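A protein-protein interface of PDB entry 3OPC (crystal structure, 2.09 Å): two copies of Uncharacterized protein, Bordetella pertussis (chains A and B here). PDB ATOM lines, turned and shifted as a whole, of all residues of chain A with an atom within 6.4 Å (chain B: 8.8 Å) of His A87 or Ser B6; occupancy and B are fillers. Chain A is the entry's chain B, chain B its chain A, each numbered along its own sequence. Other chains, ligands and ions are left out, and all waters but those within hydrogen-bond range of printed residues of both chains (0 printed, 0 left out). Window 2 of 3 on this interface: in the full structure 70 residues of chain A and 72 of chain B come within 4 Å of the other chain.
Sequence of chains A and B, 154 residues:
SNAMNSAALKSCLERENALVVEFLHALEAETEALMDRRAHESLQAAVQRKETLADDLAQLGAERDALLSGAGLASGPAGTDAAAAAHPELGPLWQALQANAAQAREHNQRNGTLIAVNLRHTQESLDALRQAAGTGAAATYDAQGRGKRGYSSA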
ATOM      1  N   LEU A  73      25.348 -11.429  14.459  1.00  0.00           N
ATOM      2  CA  LEU A  73      26.764 -11.739  14.743  1.00  0.00           C
ATOM      3  C   LEU A  73      27.693 -11.186  13.652  1.00  0.00           C
ATOM      4  O   LEU A  73      27.244 -10.931  12.543  1.00  0.00           O
ATOM      5  CB  LEU A  73      26.940 -13.259  14.850  1.00  0.00           C
ATOM      6  CG  LEU A  73      26.193 -13.943  16.001  1.00  0.00           C
ATOM      7  CD1 LEU A  73      26.209 -15.460  15.854  1.00  0.00           C
ATOM      8  CD2 LEU A  73      26.791 -13.526  17.343  1.00  0.00           C
ATOM      9  N   ALA A  82      31.746 -17.360  17.576  1.00  0.00           N
ATOM     10  CA  ALA A  82      30.694 -16.999  18.522  1.00  0.00           C
ATOM     11  C   ALA A  82      29.518 -17.961  18.416  1.00  0.00           C
ATOM     12  O   ALA A  82      28.991 -18.409  19.431  1.00  0.00           O
ATOM     13  CB  ALA A  82      30.211 -15.554  18.285  1.00  0.00           C
ATOM     14  N   ALA A  83      29.095 -18.261  17.189  1.00  0.00           N
ATOM     15  CA  ALA A  83      28.002 -19.203  16.987  1.00  0.00           C
ATOM     16  C   ALA A  83      28.326 -20.621  17.496  1.00  0.00           C
ATOM     17  O   ALA A  83      27.465 -21.258  18.086  1.00  0.00           O
ATOM     18  CB  ALA A  83      27.564 -19.237  15.538  1.00  0.00           C
ATOM     19  N   ALA A  84      29.547 -21.103  17.280  1.00  0.00           N
ATOM     20  CA  ALA A  84      29.946 -22.456  17.746  1.00  0.00           C
ATOM     21  C   ALA A  84      30.032 -22.521  19.276  1.00  0.00           C
ATOM     22  O   ALA A  84      29.718 -23.555  19.886  1.00  0.00           O
ATOM     23  CB  ALA A  84      31.269 -22.895  17.123  1.00  0.00           C
ATOM     24  N   ALA A  85      30.445 -21.412  19.884  1.00  0.00           N
ATOM     25  CA  ALA A  85      30.452 -21.267  21.341  1.00  0.00           C
ATOM     26  C   ALA A  85      29.048 -21.333  21.915  1.00  0.00           C
ATOM     27  O   ALA A  85      28.817 -22.029  22.899  1.00  0.00           O
ATOM     28  CB  ALA A  85      31.116 -19.949  21.735  1.00  0.00           C
ATOM     29  N   ALA A  86      28.115 -20.613  21.296  1.00  0.00           N
ATOM     30  CA  ALA A  86      26.727 -20.558  21.766  1.00  0.00           C
ATOM     31  C   ALA A  86      25.906 -21.805  21.419  1.00  0.00           C
ATOM     32  O   ALA A  86      24.924 -22.091  22.099  1.00  0.00           O
ATOM     33  CB  ALA A  86      26.033 -19.318  21.213  1.00  0.00           C
ATOM     34  N   HIS A  87      26.285 -22.515  20.347  1.00  0.00           N
ATOM     35  CA  HIS A  87      25.629 -23.760  19.914  1.00  0.00           C
ATOM     36  C   HIS A  87      26.675 -24.864  19.749  1.00  0.00           C
ATOM     37  O   HIS A  87      27.057 -25.175  18.627  1.00  0.00           O
ATOM     38  CB  HIS A  87      24.912 -23.570  18.571  1.00  0.00           C
ATOM     39  CG  HIS A  87      23.954 -22.428  18.557  1.00  0.00           C
ATOM     40  ND1 HIS A  87      24.315 -21.157  18.153  1.00  0.00           N
ATOM     41  CD2 HIS A  87      22.660 -22.349  18.942  1.00  0.00           C
ATOM     42  CE1 HIS A  87      23.278 -20.348  18.277  1.00  0.00           C
ATOM     43  NE2 HIS A  87      22.262 -21.047  18.756  1.00  0.00           N
ATOM     44  N   PRO A  88      27.135 -25.455  20.859  1.00  0.00           N
ATOM     45  CA  PRO A  88      28.311 -26.346  20.898  1.00  0.00           C
ATOM     46  C   PRO A  88      28.263 -27.530  19.970  1.00  0.00           C
ATOM     47  O   PRO A  88      29.304 -28.111  19.672  1.00  0.00           O
ATOM     48  CB  PRO A  88      28.306 -26.874  22.327  1.00  0.00           C
ATOM     49  CG  PRO A  88      27.588 -25.862  23.106  1.00  0.00           C
ATOM     50  CD  PRO A  88      26.548 -25.287  22.197  1.00  0.00           C
ATOM     51  N   GLU A  89      27.066 -27.915  19.549  1.00  0.00           N
ATOM     52  CA  GLU A  89      26.923 -29.013  18.598  1.00  0.00           C
ATOM     53  C   GLU A  89      27.522 -28.667  17.233  1.00  0.00           C
ATOM     54  O   GLU A  89      27.647 -29.534  16.405  1.00  0.00           O
ATOM     55  CB  GLU A  89      25.454 -29.445  18.430  1.00  0.00           C
ATOM     56  CG  GLU A  89      24.559 -28.480  17.639  1.00  0.00           C
ATOM     57  CD  GLU A  89      23.900 -27.415  18.491  1.00  0.00           C
ATOM     58  OE1 GLU A  89      24.397 -27.132  19.626  1.00  0.00           O
ATOM     59  OE2 GLU A  89      22.869 -26.857  18.017  1.00  0.00           O
ATOM     60  N   LEU A  90      27.853 -27.398  16.990  1.00  0.00           N
ATOM     61  CA  LEU A  90      28.542 -27.030  15.767  1.00  0.00           C
ATOM     62  C   LEU A  90      30.067 -27.033  15.899  1.00  0.00           C
ATOM     63  O   LEU A  90      30.755 -26.732  14.939  1.00  0.00           O
ATOM     64  CB  LEU A  90      28.106 -25.654  15.317  1.00  0.00           C
ATOM     65  CG  LEU A  90      26.615 -25.344  15.293  1.00  0.00           C
ATOM     66  CD1 LEU A  90      26.469 -23.896  14.897  1.00  0.00           C
ATOM     67  CD2 LEU A  90      25.836 -26.233  14.399  1.00  0.00           C
ATOM     68  N   GLY A  91      30.595 -27.374  17.072  1.00  0.00           N
ATOM     69  CA  GLY A  91      32.018 -27.213  17.367  1.00  0.00           C
ATOM     70  C   GLY A  91      32.912 -28.085  16.487  1.00  0.00           C
ATOM     71  O   GLY A  91      33.777 -27.550  15.779  1.00  0.00           O
ATOM     72  N   MET B   4      16.455 -20.187   9.051  1.00  0.00           N
ATOM     73  CA  MET B   4      17.544 -19.276   9.473  1.00  0.00           C
ATOM     74  C   MET B   4      17.811 -19.435  10.956  1.00  0.00           C
ATOM     75  O   MET B   4      17.382 -18.610  11.761  1.00  0.00           O
ATOM     76  CB  MET B   4      17.168 -17.834   9.172  1.00  0.00           C
ATOM     77  CG  MET B   4      17.013 -17.542   7.700  1.00  0.00           C
ATOM     78  SD  MET B   4      17.179 -15.643   7.373  1.00  0.00           S
ATOM     79  CE  MET B   4      19.003 -15.348   8.017  1.00  0.00           C
ATOM     80  N   ASN B   5      18.510 -20.509  11.314  1.00  0.00           N
ATOM     81  CA  ASN B   5      18.786 -20.818  12.716  1.00  0.00           C
ATOM     82  C   ASN B   5      20.088 -21.602  12.906  1.00  0.00           C
ATOM     83  O   ASN B   5      20.998 -21.524  12.080  1.00  0.00           O
ATOM     84  CB  ASN B   5      17.611 -21.582  13.334  1.00  0.00           C
ATOM     85  CG  ASN B   5      17.128 -22.728  12.460  1.00  0.00           C
ATOM     86  OD1 ASN B   5      17.913 -23.363  11.760  1.00  0.00           O
ATOM     87  ND2 ASN B   5      15.830 -23.003  12.510  1.00  0.00           N
ATOM     88  N   SER B   6      20.180 -22.344  14.005  1.00  0.00           N
ATOM     89  CA  SER B   6      21.380 -23.117  14.291  1.00  0.00           C
ATOM     90  C   SER B   6      21.484 -24.383  13.429  1.00  0.00           C
ATOM     91  O   SER B   6      22.594 -24.805  13.085  1.00  0.00           O
ATOM     92  CB  SER B   6      21.439 -23.494  15.768  1.00  0.00           C
ATOM     93  OG  SER B   6      21.138 -24.865  15.942  1.00  0.00           O
ATOM     94  N   ALA B   7      20.345 -24.992  13.097  1.00  0.00           N
ATOM     95  CA  ALA B   7      20.317 -26.136  12.161  1.00  0.00           C
ATOM     96  C   ALA B   7      20.674 -25.680  10.751  1.00  0.00           C
ATOM     97  O   ALA B   7      21.355 -26.408  10.009  1.00  0.00           O
ATOM     98  CB  ALA B   7      18.985 -26.832  12.159  1.00  0.00           C
ATOM     99  N   ALA B   8      20.229 -24.473  10.402  1.00  0.00           N
ATOM    100  CA  ALA B   8      20.584 -23.882   9.118  1.00  0.00           C
ATOM    101  C   ALA B   8      22.091 -23.652   9.065  1.00  0.00           C
ATOM    102  O   ALA B   8      22.704 -23.844   8.032  1.00  0.00           O
ATOM    103  CB  ALA B   8      19.847 -22.582   8.886  1.00  0.00           C
ATOM    104  N   LEU B   9      22.672 -23.209  10.167  1.00  0.00           N
ATOM    105  CA  LEU B   9      24.085 -22.912  10.170  1.00  0.00           C
ATOM    106  C   LEU B   9      24.854 -24.227  10.084  1.00  0.00           C
ATOM    107  O   LEU B   9      25.856 -24.306   9.413  1.00  0.00           O
ATOM    108  CB  LEU B   9      24.503 -22.127  11.414  1.00  0.00           C
ATOM    109  CG  LEU B   9      26.003 -21.794  11.479  1.00  0.00           C
ATOM    110  CD1 LEU B   9      26.492 -21.129  10.154  1.00  0.00           C
ATOM    111  CD2 LEU B   9      26.354 -20.963  12.700  1.00  0.00           C
ATOM    112  N   LYS B  10      24.360 -25.253  10.759  1.00  0.00           N
ATOM    113  CA  LYS B  10      24.960 -26.581  10.657  1.00  0.00           C
ATOM    114  C   LYS B  10      24.921 -27.130   9.217  1.00  0.00           C
ATOM    115  O   LYS B  10      25.890 -27.714   8.743  1.00  0.00           O
ATOM    116  CB  LYS B  10      24.243 -27.542  11.594  1.00  0.00           C
ATOM    117  CG  LYS B  10      24.934 -28.881  11.792  1.00  0.00           C
ATOM    118  CD  LYS B  10      24.000 -29.932  12.487  1.00  0.00           C
ATOM    119  CE  LYS B  10      24.802 -31.186  12.907  1.00  0.00           C
ATOM    120  NZ  LYS B  10      24.028 -32.463  12.767  1.00  0.00           N
ATOM    121  N   SER B  11      23.792 -26.966   8.539  1.00  0.00           N
ATOM    122  CA  SER B  11      23.664 -27.375   7.143  1.00  0.00           C
ATOM    123  C   SER B  11      24.723 -26.676   6.304  1.00  0.00           C
ATOM    124  O   SER B  11      25.398 -27.305   5.493  1.00  0.00           O
ATOM    125  CB  SER B  11      22.250 -27.061   6.605  1.00  0.00           C
ATOM    126  OG  SER B  11      22.190 -27.318   5.205  1.00  0.00           O
ATOM    127  N   CYS B  12      24.875 -25.371   6.520  1.00  0.00           N
ATOM    128  CA  CYS B  12      25.830 -24.591   5.751  1.00  0.00           C
ATOM    129  C   CYS B  12      27.257 -25.066   5.970  1.00  0.00           C
ATOM    130  O   CYS B  12      27.995 -25.325   5.003  1.00  0.00           O
ATOM    131  CB  CYS B  12      25.698 -23.106   6.084  1.00  0.00           C
ATOM    132  SG  CYS B  12      26.767 -21.996   5.132  1.00  0.00           S
ATOM    133  N   LEU B  13      27.642 -25.223   7.238  1.00  0.00           N
ATOM    134  CA  LEU B  13      28.965 -25.759   7.560  1.00  0.00           C
ATOM    135  C   LEU B  13      29.184 -27.127   6.917  1.00  0.00           C
ATOM    136  O   LEU B  13      30.218 -27.332   6.320  1.00  0.00           O
ATOM    137  CB  LEU B  13      29.198 -25.832   9.071  1.00  0.00           C
ATOM    138  CG  LEU B  13      29.268 -24.492   9.823  1.00  0.00           C
ATOM    139  CD1 LEU B  13      29.238 -24.670  11.343  1.00  0.00           C
ATOM    140  CD2 LEU B  13      30.467 -23.685   9.405  1.00  0.00           C
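ND1 of His A87 is in hydrogen-bond range of O of Ala A83.
The side-chain hydroxyl (OG) of Ser B6 lies within hydrogen-bond range of the side-chain carboxylate (OE2) of Glu A89 (3.4 Å).
No position is printed for both chains.
Of the 6 pairs that touch across the chains among the printed residues, none has its exchanged pair printed and touching as well.
Printed residues of chain B within 4 Å of His A87: Ser B6.
Of the printed residues of chain A, Ser B6 touches His A87, Glu A89 and Leu A90.
Of the printed residues of chain A, Leu B9 touches Ala A83 (3.5 Å) and Leu A90 (3.7 Å).
Printed residues of chain B within 4 Å of Leu A90: Ser B6, Leu B9 and Lys B10.
Of the printed residues of chain B, Ala A83 touches Leu B9 (3.5 Å).
Ala A85 touches none of the printed residues of chain B.
Ala B8 touches none of the printed residues of chain A.
The nearest printed residue of chain B that does not touch His A87 is Leu B9 (5.8 Å).
The nearest printed residue of chain A that does not touch Ser B6 is Ala A83 (6.8 Å).
The nearest printed residue of chain B that does not touch Ala A83 is Ser B6 (6.8 Å).
Leu B9 touches Ala A83.
CD2 of His A87 touches CB of Ser B6, at 3.6 Å.
Leu A90 touches Ser B6.
Leu A90 touches Leu B9.
Leu A90 touches Lys B10 (CD2 to CB, 3.5 Å).
Among the printed residues, 6 pairs touch across the chains.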
